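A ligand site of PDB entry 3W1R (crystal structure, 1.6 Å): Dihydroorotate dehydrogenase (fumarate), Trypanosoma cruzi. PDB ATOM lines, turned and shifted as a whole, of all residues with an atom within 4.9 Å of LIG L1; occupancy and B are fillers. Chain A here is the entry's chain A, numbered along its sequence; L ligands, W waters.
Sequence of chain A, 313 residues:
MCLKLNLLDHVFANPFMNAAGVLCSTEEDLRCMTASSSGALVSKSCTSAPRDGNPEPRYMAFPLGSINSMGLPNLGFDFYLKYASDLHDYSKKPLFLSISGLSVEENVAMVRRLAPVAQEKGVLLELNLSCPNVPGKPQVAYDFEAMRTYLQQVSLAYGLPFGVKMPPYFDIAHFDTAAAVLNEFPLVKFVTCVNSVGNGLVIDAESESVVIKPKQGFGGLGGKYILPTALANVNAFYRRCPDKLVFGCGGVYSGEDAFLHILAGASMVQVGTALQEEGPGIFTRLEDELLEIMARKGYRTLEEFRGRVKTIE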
ATOM      1  N   ALA A  19      23.631 -25.338  26.736  1.00  0.00           N
ATOM      2  CA  ALA A  19      23.713 -23.907  26.813  1.00  0.00           C
ATOM      3  C   ALA A  19      22.373 -23.269  26.364  1.00  0.00           C
ATOM      4  O   ALA A  19      21.731 -23.778  25.422  1.00  0.00           O
ATOM      5  CB  ALA A  19      24.861 -23.404  25.870  1.00  0.00           C
ATOM      6  N   ALA A  20      21.950 -22.184  27.026  1.00  0.00           N
ATOM      7  CA  ALA A  20      20.714 -21.548  26.549  1.00  0.00           C
ATOM      8  C   ALA A  20      20.742 -21.262  25.063  1.00  0.00           C
ATOM      9  O   ALA A  20      21.763 -20.812  24.534  1.00  0.00           O
ATOM     10  CB  ALA A  20      20.489 -20.252  27.361  1.00  0.00           C
ATOM     11  N   GLY A  21      19.612 -21.508  24.432  1.00  0.00           N
ATOM     12  CA  GLY A  21      19.518 -21.278  22.992  1.00  0.00           C
ATOM     13  C   GLY A  21      19.606 -22.557  22.163  1.00  0.00           C
ATOM     14  O   GLY A  21      19.098 -22.594  21.033  1.00  0.00           O
ATOM     15  N   VAL A  22      20.331 -23.550  22.681  1.00  0.00           N
ATOM     16  CA  VAL A  22      20.521 -24.786  21.890  1.00  0.00           C
ATOM     17  C   VAL A  22      19.628 -25.906  22.432  1.00  0.00           C
ATOM     18  O   VAL A  22      19.605 -26.179  23.637  1.00  0.00           O
ATOM     19  CB  VAL A  22      22.004 -25.216  22.016  1.00  0.00           C
ATOM     20  CG1 VAL A  22      22.217 -26.550  21.277  1.00  0.00           C
ATOM     21  CG2 VAL A  22      22.857 -24.105  21.399  1.00  0.00           C
ATOM     22  N   LYS A  44      15.210 -21.912  26.330  1.00  0.00           N
ATOM     23  CA  LYS A  44      15.601 -20.799  25.518  1.00  0.00           C
ATOM     24  C   LYS A  44      15.292 -19.453  26.181  1.00  0.00           C
ATOM     25  O   LYS A  44      14.142 -19.260  26.589  1.00  0.00           O
ATOM     26  CB  LYS A  44      14.813 -20.945  24.173  1.00  0.00           C
ATOM     27  CG  LYS A  44      14.993 -19.705  23.237  1.00  0.00           C
ATOM     28  CD  LYS A  44      16.428 -19.494  22.658  1.00  0.00           C
ATOM     29  CE  LYS A  44      16.550 -18.101  21.917  1.00  0.00           C
ATOM     30  NZ  LYS A  44      17.963 -17.752  21.349  1.00  0.00           N
ATOM     31  N   SER A  45      16.261 -18.541  26.106  1.00  0.00           N
ATOM     32  CA  SER A  45      16.044 -17.156  26.671  1.00  0.00           C
ATOM     33  C   SER A  45      14.775 -16.617  26.043  1.00  0.00           C
ATOM     34  O   SER A  45      14.602 -16.665  24.824  1.00  0.00           O
ATOM     35  CB  SER A  45      17.152 -16.206  26.293  1.00  0.00           C
ATOM     36  OG  SER A  45      18.306 -16.661  27.059  1.00  0.00           O
ATOM     37  N   TYR A  59      22.352 -18.935  11.748  1.00  0.00           N
ATOM     38  CA  TYR A  59      23.351 -19.744  12.423  1.00  0.00           C
ATOM     39  C   TYR A  59      24.086 -20.548  11.386  1.00  0.00           C
ATOM     40  O   TYR A  59      23.485 -21.168  10.459  1.00  0.00           O
ATOM     41  CB  TYR A  59      22.616 -20.722  13.421  1.00  0.00           C
ATOM     42  CG  TYR A  59      23.547 -21.840  13.960  1.00  0.00           C
ATOM     43  CD1 TYR A  59      24.314 -21.608  15.095  1.00  0.00           C
ATOM     44  CD2 TYR A  59      23.682 -23.099  13.281  1.00  0.00           C
ATOM     45  CE1 TYR A  59      25.129 -22.597  15.633  1.00  0.00           C
ATOM     46  CE2 TYR A  59      24.535 -24.085  13.788  1.00  0.00           C
ATOM     47  CZ  TYR A  59      25.287 -23.814  14.928  1.00  0.00           C
ATOM     48  OH  TYR A  59      26.082 -24.770  15.528  1.00  0.00           O
ATOM     49  N   SER A  66      30.986 -21.893  15.661  1.00  0.00           N
ATOM     50  CA  SER A  66      29.753 -21.410  15.053  1.00  0.00           C
ATOM     51  C   SER A  66      29.680 -19.854  15.208  1.00  0.00           C
ATOM     52  O   SER A  66      30.392 -19.207  15.977  1.00  0.00           O
ATOM     53  CB  SER A  66      28.559 -22.075  15.808  1.00  0.00           C
ATOM     54  OG  SER A  66      28.408 -21.557  17.151  1.00  0.00           O
ATOM     55  N   ASN A  68      26.362 -16.908  15.182  1.00  0.00           N
ATOM     56  CA  ASN A  68      24.853 -16.808  15.131  1.00  0.00           C
ATOM     57  C   ASN A  68      24.485 -15.351  15.390  1.00  0.00           C
ATOM     58  O   ASN A  68      25.002 -14.621  16.231  1.00  0.00           O
ATOM     59  CB  ASN A  68      24.178 -17.752  16.141  1.00  0.00           C
ATOM     60  CG  ASN A  68      24.084 -17.133  17.497  1.00  0.00           C
ATOM     61  OD1 ASN A  68      23.130 -16.359  17.788  1.00  0.00           O
ATOM     62  ND2 ASN A  68      24.993 -17.511  18.410  1.00  0.00           N
ATOM     63  N   MET A  70      20.706 -14.950  15.875  1.00  0.00           N
ATOM     64  CA  MET A  70      19.379 -15.492  15.881  1.00  0.00           C
ATOM     65  C   MET A  70      18.250 -14.471  16.013  1.00  0.00           C
ATOM     66  O   MET A  70      17.232 -14.600  15.419  1.00  0.00           O
ATOM     67  CB  MET A  70      19.205 -16.531  16.970  1.00  0.00           C
ATOM     68  CG  MET A  70      20.179 -17.651  17.021  1.00  0.00           C
ATOM     69  SD  MET A  70      20.217 -18.658  15.511  1.00  0.00           S
ATOM     70  CE  MET A  70      18.677 -19.591  15.655  1.00  0.00           C
ATOM     71  N   LEU A  72      16.886 -13.670  19.047  1.00  0.00           N
ATOM     72  CA  LEU A  72      16.094 -14.106  20.125  1.00  0.00           C
ATOM     73  C   LEU A  72      14.753 -14.701  19.736  1.00  0.00           C
ATOM     74  O   LEU A  72      13.773 -14.383  20.290  1.00  0.00           O
ATOM     75  CB  LEU A  72      15.908 -12.943  21.114  1.00  0.00           C
ATOM     76  CG  LEU A  72      15.572 -13.181  22.585  1.00  0.00           C
ATOM     77  CD1 LEU A  72      16.444 -14.246  23.193  1.00  0.00           C
ATOM     78  CD2 LEU A  72      15.934 -11.868  23.295  1.00  0.00           C
ATOM     79  N   SER A  98      15.727 -19.523  31.290  1.00  0.00           N
ATOM     80  CA  SER A  98      16.478 -18.292  31.004  1.00  0.00           C
ATOM     81  C   SER A  98      15.548 -17.220  30.512  1.00  0.00           C
ATOM     82  O   SER A  98      14.678 -17.475  29.695  1.00  0.00           O
ATOM     83  CB  SER A  98      17.488 -18.655  29.902  1.00  0.00           C
ATOM     84  OG  SER A  98      18.150 -17.406  29.457  1.00  0.00           O
ATOM     85  N   GLU A 126      17.938 -18.272  35.198  1.00  0.00           N
ATOM     86  CA  GLU A 126      19.225 -17.728  34.602  1.00  0.00           C
ATOM     87  C   GLU A 126      18.840 -16.448  33.853  1.00  0.00           C
ATOM     88  O   GLU A 126      18.157 -16.469  32.826  1.00  0.00           O
ATOM     89  CB  GLU A 126      19.909 -18.785  33.727  1.00  0.00           C
ATOM     90  CG  GLU A 126      21.259 -18.249  33.206  1.00  0.00           C
ATOM     91  CD  GLU A 126      22.004 -19.272  32.343  1.00  0.00           C
ATOM     92  OE1 GLU A 126      21.724 -19.371  31.118  1.00  0.00           O
ATOM     93  OE2 GLU A 126      22.839 -20.080  32.851  1.00  0.00           O
ATOM     94  N   ASN A 128      19.725 -13.523  31.442  1.00  0.00           N
ATOM     95  CA  ASN A 128      20.727 -13.240  30.446  1.00  0.00           C
ATOM     96  C   ASN A 128      21.038 -11.777  30.398  1.00  0.00           C
ATOM     97  O   ASN A 128      20.233 -10.951  29.940  1.00  0.00           O
ATOM     98  CB  ASN A 128      20.149 -13.698  29.083  1.00  0.00           C
ATOM     99  CG  ASN A 128      21.140 -13.542  27.939  1.00  0.00           C
ATOM    100  OD1 ASN A 128      22.276 -13.241  28.086  1.00  0.00           O
ATOM    101  ND2 ASN A 128      20.644 -13.943  26.766  1.00  0.00           N
ATOM    102  N   LYS A 165      23.751 -14.910  33.234  1.00  0.00           N
ATOM    103  CA  LYS A 165      24.584 -15.406  32.092  1.00  0.00           C
ATOM    104  C   LYS A 165      25.375 -14.162  31.591  1.00  0.00           C
ATOM    105  O   LYS A 165      24.792 -13.116  31.301  1.00  0.00           O
ATOM    106  CB  LYS A 165      23.626 -15.908  30.978  1.00  0.00           C
ATOM    107  CG  LYS A 165      24.354 -16.300  29.659  1.00  0.00           C
ATOM    108  CD  LYS A 165      25.104 -17.612  29.788  1.00  0.00           C
ATOM    109  CE  LYS A 165      25.538 -18.152  28.441  1.00  0.00           C
ATOM    110  NZ  LYS A 165      24.408 -18.699  27.674  1.00  0.00           N
ATOM    111  N   VAL A 194      30.674 -18.464  29.576  1.00  0.00           N
ATOM    112  CA  VAL A 194      30.332 -17.159  28.964  1.00  0.00           C
ATOM    113  C   VAL A 194      29.299 -17.393  27.892  1.00  0.00           C
ATOM    114  O   VAL A 194      29.109 -18.518  27.318  1.00  0.00           O
ATOM    115  CB  VAL A 194      31.550 -16.462  28.227  1.00  0.00           C
ATOM    116  CG1 VAL A 194      32.562 -16.101  29.356  1.00  0.00           C
ATOM    117  CG2 VAL A 194      32.188 -17.467  27.196  1.00  0.00           C
ATOM    118  N   ASN A 195      28.597 -16.293  27.591  1.00  0.00           N
ATOM    119  CA  ASN A 195      27.842 -16.203  26.320  1.00  0.00           C
ATOM    120  C   ASN A 195      28.814 -16.121  25.107  1.00  0.00           C
ATOM    121  O   ASN A 195      30.039 -16.103  25.273  1.00  0.00           O
ATOM    122  CB  ASN A 195      26.926 -14.919  26.411  1.00  0.00           C
ATOM    123  CG  ASN A 195      25.627 -15.088  25.620  1.00  0.00           C
ATOM    124  OD1 ASN A 195      25.617 -15.557  24.485  1.00  0.00           O
ATOM    125  ND2 ASN A 195      24.490 -14.799  26.310  1.00  0.00           N
ATOM    126  N   SER A 196      28.269 -16.008  23.886  1.00  0.00           N
ATOM    127  CA  SER A 196      29.167 -15.977  22.735  1.00  0.00           C
ATOM    128  C   SER A 196      30.098 -14.781  22.717  1.00  0.00           C
ATOM    129  O   SER A 196      29.841 -13.725  23.274  1.00  0.00           O
ATOM    130  CB  SER A 196      28.323 -16.019  21.427  1.00  0.00           C
ATOM    131  OG  SER A 196      27.224 -15.245  21.471  1.00  0.00           O
ATOM    132  N   GLY A 222      30.821 -19.102  18.917  1.00  0.00           N
ATOM    133  CA  GLY A 222      30.956 -20.202  19.862  1.00  0.00           C
ATOM    134  C   GLY A 222      31.892 -21.267  19.356  1.00  0.00           C
ATOM    135  O   GLY A 222      32.330 -21.216  18.186  1.00  0.00           O
ATOM    136  N   GLY A 223      32.160 -22.225  20.249  1.00  0.00           N
ATOM    137  CA  GLY A 223      32.886 -23.416  19.883  1.00  0.00           C
ATOM    138  C   GLY A 223      34.393 -23.347  20.152  1.00  0.00           C
ATOM    139  O   GLY A 223      34.796 -22.652  21.069  1.00  0.00           O
ATOM    140  N   ILE A 226      36.553 -20.232  21.151  1.00  0.00           N
ATOM    141  CA  ILE A 226      36.327 -19.424  22.422  1.00  0.00           C
ATOM    142  C   ILE A 226      36.723 -20.141  23.692  1.00  0.00           C
ATOM    143  O   ILE A 226      36.542 -19.575  24.732  1.00  0.00           O
ATOM    144  CB  ILE A 226      34.872 -18.914  22.525  1.00  0.00           C
ATOM    145  CG1 ILE A 226      33.803 -20.003  22.925  1.00  0.00           C
ATOM    146  CG2 ILE A 226      34.452 -18.220  21.217  1.00  0.00           C
ATOM    147  CD1 ILE A 226      32.528 -19.286  23.459  1.00  0.00           C
ATOM    148  N   CYS A 249      30.682 -22.209  30.368  1.00  0.00           N
ATOM    149  CA  CYS A 249      30.107 -22.448  29.028  1.00  0.00           C
ATOM    150  C   CYS A 249      31.085 -21.879  27.995  1.00  0.00           C
ATOM    151  O   CYS A 249      31.590 -20.790  28.189  1.00  0.00           O
ATOM    152  CB  CYS A 249      28.735 -21.724  28.973  1.00  0.00           C
ATOM    153  SG  CYS A 249      27.847 -21.976  27.387  1.00  0.00           S
ATOM    154  N   GLY A 250      31.398 -22.623  26.971  1.00  0.00           N
ATOM    155  CA  GLY A 250      32.190 -22.130  25.801  1.00  0.00           C
ATOM    156  C   GLY A 250      33.218 -23.163  25.423  1.00  0.00           C
ATOM    157  O   GLY A 250      34.116 -23.523  26.201  1.00  0.00           O
ATOM    158  N   GLY A 251      33.084 -23.648  24.180  1.00  0.00           N
ATOM    159  CA  GLY A 251      34.177 -24.477  23.681  1.00  0.00           C
ATOM    160  C   GLY A 251      34.184 -25.880  24.185  1.00  0.00           C
ATOM    161  O   GLY A 251      35.195 -26.565  23.977  1.00  0.00           O
ATOM    162  N   VAL A 252      33.098 -26.367  24.824  1.00  0.00           N
ATOM    163  CA  VAL A 252      33.159 -27.793  25.289  1.00  0.00           C
ATOM    164  C   VAL A 252      32.730 -28.708  24.172  1.00  0.00           C
ATOM    165  O   VAL A 252      31.556 -28.699  23.768  1.00  0.00           O
ATOM    166  CB  VAL A 252      32.248 -27.981  26.566  1.00  0.00           C
ATOM    167  CG1 VAL A 252      32.210 -29.446  26.985  1.00  0.00           C
ATOM    168  CG2 VAL A 252      32.769 -27.061  27.679  1.00  0.00           C
ATOM    169  N   GLN A 270      28.092 -26.160  30.599  1.00  0.00           N
ATOM    170  CA  GLN A 270      27.035 -26.068  29.553  1.00  0.00           C
ATOM    171  C   GLN A 270      27.677 -26.306  28.149  1.00  0.00           C
ATOM    172  O   GLN A 270      28.887 -25.937  27.941  1.00  0.00           O
ATOM    173  CB  GLN A 270      26.439 -24.627  29.552  1.00  0.00           C
ATOM    174  CG  GLN A 270      25.984 -24.279  31.000  1.00  0.00           C
ATOM    175  CD  GLN A 270      25.099 -23.016  30.941  1.00  0.00           C
ATOM    176  OE1 GLN A 270      25.251 -22.193  30.000  1.00  0.00           O
ATOM    177  NE2 GLN A 270      24.218 -22.850  31.931  1.00  0.00           N
ATOM    178  N   VAL A 271      26.884 -26.805  27.218  1.00  0.00           N
ATOM    179  CA  VAL A 271      27.356 -27.246  25.899  1.00  0.00           C
ATOM    180  C   VAL A 271      26.463 -26.636  24.872  1.00  0.00           C
ATOM    181  O   VAL A 271      25.264 -26.958  24.898  1.00  0.00           O
ATOM    182  CB  VAL A 271      27.354 -28.783  25.782  1.00  0.00           C
ATOM    183  CG1 VAL A 271      28.036 -29.178  24.465  1.00  0.00           C
ATOM    184  CG2 VAL A 271      28.065 -29.444  27.022  1.00  0.00           C
ATOM    185  N   GLY A 272      26.990 -25.744  24.026  1.00  0.00           N
ATOM    186  CA  GLY A 272      26.175 -25.028  23.013  1.00  0.00           C
ATOM    187  C   GLY A 272      26.543 -25.611  21.644  1.00  0.00           C
ATOM    188  O   GLY A 272      25.917 -26.596  21.216  1.00  0.00           O
ATOM    189  N   THR A 273      27.492 -24.977  20.955  1.00  0.00           N
ATOM    190  CA  THR A 273      27.816 -25.405  19.574  1.00  0.00           C
ATOM    191  C   THR A 273      28.002 -26.905  19.392  1.00  0.00           C
ATOM    192  O   THR A 273      27.389 -27.481  18.486  1.00  0.00           O
ATOM    193  CB  THR A 273      29.128 -24.680  19.140  1.00  0.00           C
ATOM    194  OG1 THR A 273      28.894 -23.273  19.178  1.00  0.00           O
ATOM    195  CG2 THR A 273      29.514 -25.037  17.718  1.00  0.00           C
ATOM    196  N   ALA A 274      28.754 -27.567  20.282  1.00  0.00           N
ATOM    197  CA  ALA A 274      28.982 -29.009  20.054  1.00  0.00           C
ATOM    198  C   ALA A 274      27.691 -29.812  20.119  1.00  0.00           C
ATOM    199  O   ALA A 274      27.603 -30.836  19.466  1.00  0.00           O
ATOM    200  CB  ALA A 274      30.004 -29.516  21.131  1.00  0.00           C
HETATM  201  N1  LIG L   1      22.831 -17.694  25.166  1.00  0.00           N
HETATM  202  C1  LIG L   1      21.822 -17.196  25.945  1.00  0.00           C
HETATM  203  O1  LIG L   1      22.069 -16.963  27.136  1.00  0.00           O
HETATM  204  N2  LIG L   1      20.529 -17.156  25.529  1.00  0.00           N
HETATM  205  C2  LIG L   1      20.166 -17.535  24.267  1.00  0.00           C
HETATM  206  O2  LIG L   1      18.950 -17.487  23.855  1.00  0.00           O
HETATM  207  C3  LIG L   1      21.189 -18.065  23.374  1.00  0.00           C
HETATM  208  N3  LIG L   1      20.882 -18.415  22.132  1.00  0.00           N
HETATM  209  C4  LIG L   1      21.818 -19.070  21.398  1.00  0.00           C
HETATM  210  C5  LIG L   1      21.451 -19.656  20.159  1.00  0.00           C
HETATM  211  C6  LIG L   1      22.415 -20.287  19.390  1.00  0.00           C
HETATM  212  C7  LIG L   1      22.036 -20.879  18.040  1.00  0.00           C
HETATM  213  C8  LIG L   1      23.784 -20.410  19.881  1.00  0.00           C
HETATM  214  C9  LIG L   1      24.840 -21.084  19.065  1.00  0.00           C
HETATM  215  C10 LIG L   1      24.147 -19.843  21.131  1.00  0.00           C
HETATM  216  C11 LIG L   1      23.198 -19.193  21.869  1.00  0.00           C
HETATM  217  N4  LIG L   1      23.518 -18.600  23.114  1.00  0.00           N
HETATM  218  C12 LIG L   1      22.545 -18.087  23.907  1.00  0.00           C
HETATM  219  C13 LIG L   1      24.869 -18.712  23.641  1.00  0.00           C
HETATM  220  C14 LIG L   1      25.209 -20.104  24.172  1.00  0.00           C
HETATM  221  O3  LIG L   1      24.375 -20.250  25.335  1.00  0.00           O
HETATM  222  C15 LIG L   1      26.613 -20.217  24.660  1.00  0.00           C
HETATM  223  O4  LIG L   1      26.858 -19.173  25.643  1.00  0.00           O
HETATM  224  C16 LIG L   1      27.611 -19.885  23.489  1.00  0.00           C
HETATM  225  O5  LIG L   1      27.161 -20.547  22.265  1.00  0.00           O
HETATM  226  C17 LIG L   1      29.034 -20.427  23.834  1.00  0.00           C
HETATM  227  O6  LIG L   1      29.054 -21.841  24.134  1.00  0.00           O
HETATM  228  P1  LIG L   1      29.603 -22.898  23.017  1.00  0.00           P
HETATM  229  O7  LIG L   1      29.369 -24.267  23.643  1.00  0.00           O
HETATM  230  O8  LIG L   1      31.021 -22.513  22.728  1.00  0.00           O
HETATM  231  O9  LIG L   1      28.699 -22.676  21.768  1.00  0.00           O
HETATM  232  O1  LG2 L   2      19.239 -15.068  20.005  1.00  0.00           O
HETATM  233  C1  LG2 L   2      20.386 -14.606  19.850  1.00  0.00           C
HETATM  234  O2  LG2 L   2      20.929 -14.076  18.863  1.00  0.00           O
HETATM  235  C2  LG2 L   2      21.409 -14.859  20.997  1.00  0.00           C
HETATM  236  N1  LG2 L   2      22.579 -15.537  20.513  1.00  0.00           N
HETATM  237  C3  LG2 L   2      23.639 -15.749  21.385  1.00  0.00           C
HETATM  238  O3  LG2 L   2      24.686 -16.316  21.026  1.00  0.00           O
HETATM  239  N2  LG2 L   2      23.477 -15.388  22.714  1.00  0.00           N
HETATM  240  C4  LG2 L   2      22.325 -14.709  23.206  1.00  0.00           C
HETATM  241  O4  LG2 L   2      22.251 -14.375  24.383  1.00  0.00           O
HETATM  242  C5  LG2 L   2      21.291 -14.440  22.280  1.00  0.00           C
HETATM  243  C6  LG2 L   2      20.116 -13.770  22.706  1.00  0.00           C
HETATM  244  C7  LG2 L   2      20.470 -12.252  23.017  1.00  0.00           C
HETATM  245  C8  LG2 L   2      20.788 -11.542  21.908  1.00  0.00           C
HETATM  246  C9  LG2 L   2      19.673 -11.129  21.135  1.00  0.00           C
HETATM  247  C10 LG2 L   2      20.068 -10.339  20.023  1.00  0.00           C
HETATM  248  C11 LG2 L   2      21.382 -10.002  19.654  1.00  0.00           C
HETATM  249  C12 LG2 L   2      22.547 -10.406  20.393  1.00  0.00           C
HETATM  250  C13 LG2 L   2      22.160 -11.184  21.555  1.00  0.00           C
HETATM  251  O   HOH W   1      18.101 -20.319  19.566  1.00  0.00           O
HETATM  252  O   HOH W   2      20.739 -17.316  29.686  1.00  0.00           O
HETATM  253  O   HOH W   3      30.548 -25.126  25.885  1.00  0.00           O
HETATM  254  O   HOH W   4      30.358 -26.431  22.390  1.00  0.00           O
HETATM  255  O   HOH W   5      27.523 -18.701  20.522  1.00  0.00           O
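Water W4 lies within hydrogen-bond range of an oxygen (O7) of LIG L1, the backbone NH (N) of Ala 274 and the backbone carbonyl oxygen (O) of Val 252.
Water W2 lies within hydrogen-bond range of OG of Ser 98, OE1 of Glu 126 and O1 of LIG L1.
Water W1 bridges the backbone carbonyl oxygen (O) of Gly 21 (2.9 Å) and the side-chain amino group (NZ) of Lys 44 (3.1 Å).
The backbone NH of Thr 273 lies within hydrogen-bond range of an oxygen (O9) of LIG L1.
The side-chain hydroxyl (OG1) of Thr 273 is in hydrogen-bond range of an oxygen (O9) of LIG L1, at 2.7 Å.
The side-chain amino group of Lys 44 lies within hydrogen-bond range of an oxygen (O2) of LIG L1, at 2.7 Å.
N of Gly 223 is in hydrogen-bond range of O8 of LIG L1.
The side-chain hydroxyl (OG) of Ser 45 is in hydrogen-bond range of a nitrogen (N2) of LIG L1, 2.7 Å away.
The backbone NH (N) of Gly 251 sits at hydrogen-bond distance from an oxygen (O8) of LIG L1 (2.8 Å).
O3 of LIG L1 is in hydrogen-bond range of O of Ala 20 (2.8 Å).
The side-chain amino group (NZ) of Lys 165 lies within hydrogen-bond range of an oxygen (O3) of LIG L1 (2.8 Å).
O7 of LIG L1 is in hydrogen-bond range of N of Gly 272 (2.8 Å).
O of Val 194 is in hydrogen-bond range of O4 of LIG L1 (2.9 Å).
The side-chain amide nitrogen (ND2) of Asn 195 lies within hydrogen-bond range of an oxygen (O1) of LIG L1, 3.4 Å away.
The side-chain amide nitrogen of Asn 128 lies within hydrogen-bond range of an oxygen (O1) of LIG L1.
The side-chain sulfur of Cys 249 lies within hydrogen-bond range of an oxygen (O4) of LIG L1.
NZ of Lys 44 is in salt-bridge range of O1 of LG2 L2, 3.3 Å away.
The side-chain amide oxygen (OD1) of Asn 195 sits at hydrogen-bond distance from a nitrogen (N2) of LG2 L2 (2.8 Å).
The side-chain amide nitrogen (ND2) of Asn 128 sits at hydrogen-bond distance from an oxygen (O4) of LG2 L2, at 2.9 Å.
ND2 of Asn 68 is in hydrogen-bond range of O3 of LG2 L2, 2.9 Å away.
N of Met 70 lies within hydrogen-bond range of O2 of LG2 L2 (3.1 Å).
O3 of LG2 L2 lies within hydrogen-bond range of OG of Ser 196.
The backbone NH (N) of Leu 72 is in hydrogen-bond range of an oxygen (O1) of LG2 L2 (2.9 Å).
Ala 19 touches LIG L1.
CA of Gly 21 touches N3 of LIG L1, at 3.3 Å.
Tyr 59 touches LIG L1 (CE1 to C9, 3.8 Å).
Asn 68 touches LIG L1.
Met 70 touches LIG L1.
Ser 196 touches LIG L1 (N to O4, 3.9 Å).
CA of Gly 222 touches O8 of LIG L1 (3.7 Å).
Ile 226 touches LIG L1 (CD1 to O8, 3.6 Å).
Gly 250 touches LIG L1 (CA to O8, 3.3 Å).
Val 271 touches LIG L1.
Hydrophobic or aromatic side chains within 4 Å of LIG L1: Ala 19, Ala 20, Tyr 59, Met 70 and Ile 226.
OG1 of Thr 273 lies within hydrogen-bond range of OG of Ser 66 (2.7 Å).
The backbone carbonyl oxygen of Cys 249 is in hydrogen-bond range of the backbone NH of Val 194 (2.9 Å).
The side-chain amide oxygen of Asn 128 sits at hydrogen-bond distance from the side-chain amide nitrogen of Asn 195 (3.2 Å).
OD1 of Asn 195 is in hydrogen-bond range of OG of Ser 196.
The backbone NH of Ala 19 is in hydrogen-bond range of the backbone carbonyl oxygen of Val 271 (2.9 Å).
OE1 of Gln 270 lies close to SG of Cys 249 (3.7 Å).
The side-chain amide oxygen of Asn 68 sits close to the backbone NH of Met 70 (3.4 Å).
The backbone carbonyl oxygen (O) of Gly 222 lies within hydrogen-bond range of the backbone NH (N) of Ser 66 (2.9 Å).
A nitrogen (N2) of LG2 L2 lies close to a nitrogen (N1) of LIG L1 (3.4 Å).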
